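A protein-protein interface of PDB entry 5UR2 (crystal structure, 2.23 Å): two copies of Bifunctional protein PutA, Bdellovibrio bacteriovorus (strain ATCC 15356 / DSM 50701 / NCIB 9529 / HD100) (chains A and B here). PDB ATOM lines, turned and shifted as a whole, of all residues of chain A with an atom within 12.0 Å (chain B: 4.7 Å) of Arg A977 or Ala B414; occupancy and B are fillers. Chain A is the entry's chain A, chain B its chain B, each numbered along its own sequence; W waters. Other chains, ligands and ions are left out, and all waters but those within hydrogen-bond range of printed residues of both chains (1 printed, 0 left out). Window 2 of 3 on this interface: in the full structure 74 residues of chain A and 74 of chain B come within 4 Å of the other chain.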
ATOM      1  N   GLY A 622      -1.867 -23.426   6.700  1.00  0.00           N
ATOM      2  CA  GLY A 622      -1.682 -22.717   7.950  1.00  0.00           C
ATOM      3  C   GLY A 622      -2.754 -21.701   8.276  1.00  0.00           C
ATOM      4  O   GLY A 622      -2.673 -21.058   9.330  1.00  0.00           O
ATOM      5  N   ASN A 973      -6.061 -18.894  12.012  1.00  0.00           N
ATOM      6  CA  ASN A 973      -4.673 -19.313  11.950  1.00  0.00           C
ATOM      7  C   ASN A 973      -4.526 -20.675  12.636  1.00  0.00           C
ATOM      8  O   ASN A 973      -4.819 -20.806  13.831  1.00  0.00           O
ATOM      9  CB  ASN A 973      -3.815 -18.248  12.622  1.00  0.00           C
ATOM     10  CG  ASN A 973      -2.365 -18.653  12.760  1.00  0.00           C
ATOM     11  OD1 ASN A 973      -1.902 -19.617  12.143  1.00  0.00           O
ATOM     12  ND2 ASN A 973      -1.632 -17.910  13.580  1.00  0.00           N
ATOM     13  N   THR A 974      -4.063 -21.689  11.892  1.00  0.00           N
ATOM     14  CA  THR A 974      -3.883 -23.025  12.454  1.00  0.00           C
ATOM     15  C   THR A 974      -2.422 -23.346  12.767  1.00  0.00           C
ATOM     16  O   THR A 974      -2.135 -24.438  13.263  1.00  0.00           O
ATOM     17  CB  THR A 974      -4.448 -24.102  11.516  1.00  0.00           C
ATOM     18  OG1 THR A 974      -3.677 -24.170  10.303  1.00  0.00           O
ATOM     19  CG2 THR A 974      -5.893 -23.810  11.186  1.00  0.00           C
ATOM     20  N   LEU A 975      -1.509 -22.410  12.520  1.00  0.00           N
ATOM     21  CA  LEU A 975      -0.080 -22.613  12.729  1.00  0.00           C
ATOM     22  C   LEU A 975       0.303 -22.253  14.163  1.00  0.00           C
ATOM     23  O   LEU A 975       0.099 -21.115  14.596  1.00  0.00           O
ATOM     24  CB  LEU A 975       0.704 -21.764  11.733  1.00  0.00           C
ATOM     25  CG  LEU A 975       2.211 -21.560  11.894  1.00  0.00           C
ATOM     26  CD1 LEU A 975       2.969 -22.880  11.801  1.00  0.00           C
ATOM     27  CD2 LEU A 975       2.686 -20.607  10.798  1.00  0.00           C
ATOM     28  N   ARG A 976       0.849 -23.228  14.894  1.00  0.00           N
ATOM     29  CA  ARG A 976       1.330 -23.047  16.260  1.00  0.00           C
ATOM     30  C   ARG A 976       2.630 -23.827  16.409  1.00  0.00           C
ATOM     31  O   ARG A 976       2.681 -25.014  16.058  1.00  0.00           O
ATOM     32  CB  ARG A 976       0.303 -23.538  17.295  1.00  0.00           C
ATOM     33  CG  ARG A 976      -1.041 -22.784  17.283  1.00  0.00           C
ATOM     34  CD  ARG A 976      -1.968 -23.260  18.395  1.00  0.00           C
ATOM     35  NE  ARG A 976      -3.382 -23.016  18.103  1.00  0.00           N
ATOM     36  CZ  ARG A 976      -4.389 -23.516  18.821  1.00  0.00           C
ATOM     37  NH1 ARG A 976      -4.147 -24.294  19.874  1.00  0.00           N
ATOM     38  NH2 ARG A 976      -5.643 -23.271  18.477  1.00  0.00           N
ATOM     39  N   ARG A 977       3.669 -23.164  16.927  1.00  0.00           N
ATOM     40  CA  ARG A 977       4.986 -23.779  17.146  1.00  0.00           C
ATOM     41  C   ARG A 977       5.559 -24.392  15.867  1.00  0.00           C
ATOM     42  O   ARG A 977       6.135 -25.482  15.899  1.00  0.00           O
ATOM     43  CB  ARG A 977       4.943 -24.859  18.236  1.00  0.00           C
ATOM     44  CG  ARG A 977       4.660 -24.370  19.621  1.00  0.00           C
ATOM     45  CD  ARG A 977       5.606 -23.285  19.998  1.00  0.00           C
ATOM     46  NE  ARG A 977       5.038 -22.516  21.088  1.00  0.00           N
ATOM     47  CZ  ARG A 977       5.124 -21.201  21.184  1.00  0.00           C
ATOM     48  NH1 ARG A 977       5.749 -20.515  20.239  1.00  0.00           N
ATOM     49  NH2 ARG A 977       4.575 -20.576  22.217  1.00  0.00           N
ATOM     50  N   GLY A 978       5.383 -23.712  14.735  1.00  0.00           N
ATOM     51  CA  GLY A 978       5.927 -24.213  13.486  1.00  0.00           C
ATOM     52  C   GLY A 978       5.166 -25.371  12.879  1.00  0.00           C
ATOM     53  O   GLY A 978       5.688 -26.041  11.983  1.00  0.00           O
ATOM     54  N   PHE A 979       3.924 -25.601  13.300  1.00  0.00           N
ATOM     55  CA  PHE A 979       3.153 -26.734  12.816  1.00  0.00           C
ATOM     56  C   PHE A 979       1.706 -26.381  12.533  1.00  0.00           C
ATOM     57  O   PHE A 979       1.044 -25.717  13.336  1.00  0.00           O
ATOM     58  CB  PHE A 979       3.212 -27.858  13.856  1.00  0.00           C
ATOM     59  CG  PHE A 979       2.106 -28.840  13.741  1.00  0.00           C
ATOM     60  CD1 PHE A 979       2.113 -29.806  12.741  1.00  0.00           C
ATOM     61  CD2 PHE A 979       1.074 -28.830  14.664  1.00  0.00           C
ATOM     62  CE1 PHE A 979       1.087 -30.722  12.635  1.00  0.00           C
ATOM     63  CE2 PHE A 979       0.044 -29.746  14.568  1.00  0.00           C
ATOM     64  CZ  PHE A 979       0.052 -30.697  13.553  1.00  0.00           C
ATOM     65  N   ALA A 980       1.202 -26.888  11.405  1.00  0.00           N
ATOM     66  CA  ALA A 980      -0.181 -26.730  11.037  1.00  0.00           C
ATOM     67  C   ALA A 980      -0.701 -28.069  10.538  1.00  0.00           C
ATOM     68  O   ALA A 980       0.010 -28.794   9.826  1.00  0.00           O
ATOM     69  CB  ALA A 980      -0.379 -25.657   9.954  1.00  0.00           C
ATOM     70  N   PRO A 981      -1.922 -28.425  10.903  1.00  0.00           N
ATOM     71  CA  PRO A 981      -2.512 -29.670  10.401  1.00  0.00           C
ATOM     72  C   PRO A 981      -2.823 -29.556   8.920  1.00  0.00           C
ATOM     73  O   PRO A 981      -3.090 -28.468   8.403  1.00  0.00           O
ATOM     74  CB  PRO A 981      -3.803 -29.814  11.217  1.00  0.00           C
ATOM     75  CG  PRO A 981      -3.761 -28.709  12.272  1.00  0.00           C
ATOM     76  CD  PRO A 981      -2.833 -27.658  11.765  1.00  0.00           C
ATOM     77  N   ASP B  58       1.305 -27.528  24.069  1.00  0.00           N
ATOM     78  CA  ASP B  58       1.672 -26.127  23.863  1.00  0.00           C
ATOM     79  C   ASP B  58       1.034 -25.213  24.905  1.00  0.00           C
ATOM     80  O   ASP B  58       1.703 -24.347  25.484  1.00  0.00           O
ATOM     81  CB  ASP B  58       1.249 -25.689  22.458  1.00  0.00           C
ATOM     82  CG  ASP B  58       1.534 -24.215  22.183  1.00  0.00           C
ATOM     83  OD1 ASP B  58       2.679 -23.793  22.437  1.00  0.00           O
ATOM     84  OD2 ASP B  58       0.626 -23.489  21.704  1.00  0.00           O
ATOM     85  N   ILE B 410       7.541 -22.221  30.207  1.00  0.00           N
ATOM     86  CA  ILE B 410       6.783 -21.788  29.036  1.00  0.00           C
ATOM     87  C   ILE B 410       7.616 -21.861  27.757  1.00  0.00           C
ATOM     88  O   ILE B 410       7.187 -22.541  26.816  1.00  0.00           O
ATOM     89  CB  ILE B 410       6.174 -20.392  29.251  1.00  0.00           C
ATOM     90  CG1 ILE B 410       4.984 -20.483  30.204  1.00  0.00           C
ATOM     91  CG2 ILE B 410       5.763 -19.776  27.935  1.00  0.00           C
ATOM     92  CD1 ILE B 410       4.035 -19.346  30.062  1.00  0.00           C
ATOM     93  N   PRO B 411       8.789 -21.223  27.641  1.00  0.00           N
ATOM     94  CA  PRO B 411       9.618 -21.513  26.449  1.00  0.00           C
ATOM     95  C   PRO B 411      10.078 -22.965  26.392  1.00  0.00           C
ATOM     96  O   PRO B 411      10.288 -23.507  25.296  1.00  0.00           O
ATOM     97  CB  PRO B 411      10.800 -20.540  26.578  1.00  0.00           C
ATOM     98  CG  PRO B 411      10.312 -19.458  27.515  1.00  0.00           C
ATOM     99  CD  PRO B 411       9.392 -20.164  28.475  1.00  0.00           C
ATOM    100  N   GLY B 412      10.220 -23.617  27.550  1.00  0.00           N
ATOM    101  CA  GLY B 412      10.622 -25.015  27.570  1.00  0.00           C
ATOM    102  C   GLY B 412       9.583 -25.962  27.001  1.00  0.00           C
ATOM    103  O   GLY B 412       9.933 -26.978  26.385  1.00  0.00           O
ATOM    104  N   MET B 413       8.300 -25.645  27.184  1.00  0.00           N
ATOM    105  CA  MET B 413       7.236 -26.430  26.579  1.00  0.00           C
ATOM    106  C   MET B 413       7.081 -26.129  25.097  1.00  0.00           C
ATOM    107  O   MET B 413       6.585 -26.985  24.360  1.00  0.00           O
ATOM    108  CB  MET B 413       5.913 -26.189  27.305  1.00  0.00           C
ATOM    109  CG  MET B 413       5.212 -27.465  27.742  1.00  0.00           C
ATOM    110  SD  MET B 413       6.183 -28.478  28.885  1.00  0.00           S
ATOM    111  CE  MET B 413       6.680 -27.261  30.110  1.00  0.00           C
ATOM    112  N   ALA B 414       7.488 -24.937  24.647  1.00  0.00           N
ATOM    113  CA  ALA B 414       7.574 -24.684  23.212  1.00  0.00           C
ATOM    114  C   ALA B 414       8.657 -25.551  22.569  1.00  0.00           C
ATOM    115  O   ALA B 414       8.419 -26.195  21.539  1.00  0.00           O
ATOM    116  CB  ALA B 414       7.832 -23.200  22.952  1.00  0.00           C
ATOM    117  N   TYR B 415       9.859 -25.575  23.171  1.00  0.00           N
ATOM    118  CA  TYR B 415      10.972 -26.372  22.650  1.00  0.00           C
ATOM    119  C   TYR B 415      10.623 -27.857  22.587  1.00  0.00           C
ATOM    120  O   TYR B 415      10.931 -28.530  21.596  1.00  0.00           O
ATOM    121  CB  TYR B 415      12.206 -26.127  23.514  1.00  0.00           C
ATOM    122  CG  TYR B 415      13.471 -26.850  23.097  1.00  0.00           C
ATOM    123  CD1 TYR B 415      14.308 -26.339  22.117  1.00  0.00           C
ATOM    124  CD2 TYR B 415      13.839 -28.032  23.712  1.00  0.00           C
ATOM    125  CE1 TYR B 415      15.475 -27.005  21.757  1.00  0.00           C
ATOM    126  CE2 TYR B 415      14.995 -28.700  23.357  1.00  0.00           C
ATOM    127  CZ  TYR B 415      15.810 -28.184  22.386  1.00  0.00           C
ATOM    128  OH  TYR B 415      16.956 -28.872  22.061  1.00  0.00           O
ATOM    129  N   LEU B 416       9.989 -28.387  23.644  1.00  0.00           N
ATOM    130  CA  LEU B 416       9.513 -29.768  23.645  1.00  0.00           C
ATOM    131  C   LEU B 416       8.567 -30.039  22.472  1.00  0.00           C
ATOM    132  O   LEU B 416       8.502 -31.171  21.970  1.00  0.00           O
ATOM    133  CB  LEU B 416       8.811 -30.078  24.971  1.00  0.00           C
ATOM    134  CG  LEU B 416       8.052 -31.417  25.151  1.00  0.00           C
ATOM    135  CD1 LEU B 416       8.999 -32.624  25.230  1.00  0.00           C
ATOM    136  CD2 LEU B 416       7.080 -31.420  26.348  1.00  0.00           C
ATOM    137  N   VAL B 417       7.799 -29.031  22.050  1.00  0.00           N
ATOM    138  CA  VAL B 417       6.898 -29.213  20.916  1.00  0.00           C
ATOM    139  C   VAL B 417       7.695 -29.355  19.633  1.00  0.00           C
ATOM    140  O   VAL B 417       7.339 -30.148  18.752  1.00  0.00           O
ATOM    141  CB  VAL B 417       5.885 -28.053  20.815  1.00  0.00           C
ATOM    142  CG1 VAL B 417       5.181 -28.094  19.467  1.00  0.00           C
ATOM    143  CG2 VAL B 417       4.855 -28.148  21.921  1.00  0.00           C
ATOM    144  N   ARG B 418       8.794 -28.604  19.513  1.00  0.00           N
ATOM    145  CA  ARG B 418       9.645 -28.718  18.326  1.00  0.00           C
ATOM    146  C   ARG B 418      10.327 -30.088  18.264  1.00  0.00           C
ATOM    147  O   ARG B 418      10.426 -30.685  17.184  1.00  0.00           O
ATOM    148  CB  ARG B 418      10.671 -27.580  18.307  1.00  0.00           C
ATOM    149  CG  ARG B 418      11.352 -27.339  16.946  1.00  0.00           C
ATOM    150  CD  ARG B 418      11.519 -25.833  16.627  1.00  0.00           C
ATOM    151  NE  ARG B 418      12.908 -25.373  16.741  1.00  0.00           N
ATOM    152  CZ  ARG B 418      13.295 -24.092  16.755  1.00  0.00           C
ATOM    153  NH1 ARG B 418      12.397 -23.114  16.667  1.00  0.00           N
ATOM    154  NH2 ARG B 418      14.589 -23.785  16.867  1.00  0.00           N
ATOM    155  N   LEU B 421       7.746 -32.506  17.075  1.00  0.00           N
ATOM    156  CA  LEU B 421       7.521 -32.355  15.642  1.00  0.00           C
ATOM    157  C   LEU B 421       8.621 -33.033  14.834  1.00  0.00           C
ATOM    158  O   LEU B 421       8.336 -33.820  13.926  1.00  0.00           O
ATOM    159  CB  LEU B 421       7.438 -30.876  15.277  1.00  0.00           C
ATOM    160  CG  LEU B 421       6.108 -30.247  15.693  1.00  0.00           C
ATOM    161  CD1 LEU B 421       6.169 -28.741  15.530  1.00  0.00           C
ATOM    162  CD2 LEU B 421       4.977 -30.847  14.882  1.00  0.00           C
ATOM    163  N   ASP B 760      -1.785 -17.323  23.700  1.00  0.00           N
ATOM    164  CA  ASP B 760      -0.349 -17.233  23.443  1.00  0.00           C
ATOM    165  C   ASP B 760       0.010 -15.755  23.386  1.00  0.00           C
ATOM    166  O   ASP B 760      -0.323 -15.069  22.412  1.00  0.00           O
ATOM    167  CB  ASP B 760      -0.009 -17.942  22.129  1.00  0.00           C
ATOM    168  CG  ASP B 760       1.503 -18.003  21.844  1.00  0.00           C
ATOM    169  OD1 ASP B 760       2.226 -17.015  22.103  1.00  0.00           O
ATOM    170  OD2 ASP B 760       1.960 -19.055  21.334  1.00  0.00           O
HETATM  171  O   HOH W   1      -1.876 -24.752  21.354  1.00  0.00           O
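No position is printed for both chains.
Of the 6 pairs that touch across the chains among the printed residues, none has its exchanged pair printed and touching as well.
NE of Arg A977 lies within salt-bridge range of OD1 of Asp B58 (3.0 Å).
The side-chain carboxylate (OD2) of Asp B760 is in salt-bridge range of the guanidinium group (NH2) of Arg A977, 3.2 Å away.
Water W1 bridges the guanidinium group (NH1) of Arg A976 (2.7 Å) and the side-chain carboxylate (OD2) of Asp B58 (2.8 Å).
Among the printed residues, pairs that only touch across the chains: Arg A977 with Leu B421, Arg A977 with Ala B414, Arg A977 with Val B417 and Phe A979 with Leu B421.
Of chain B, only Asp B58 (3.0 Å), Ala B414 (3.4 Å), Val B417 (3.5 Å), Leu B421 (3.3 Å) and Asp B760 (3.2 Å) come within 4 Å of Arg A977.
Printed residues of chain B within 4 Å of Phe A979: Leu B421 (3.5 Å).
Of chain A, only Arg A977 comes within 4 Å of Asp B58.
No residue of chain A comes within 4 Å of Pro B411.
No residue of chain A comes within 4 Å of Met B413.
Of chain A, only Arg A977 (3.4 Å) comes within 4 Å of Ala B414.
No residue of chain A comes within 4 Å of Leu B416.
Of chain A, only Arg A977 comes within 4 Å of Val B417.
Of the printed residues of chain A, Leu B421 touches Arg A977 (3.3 Å) and Phe A979 (3.5 Å).
Asp B760 touches one residue of chain A.
The nearest printed residue of chain B that does not touch Arg A977 is Arg B418 (5.4 Å).
Hydrophobic or aromatic side chains of chain A that line the printed part of chain B: Phe A979.
Among the printed residues, 6 pairs touch across the chains.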
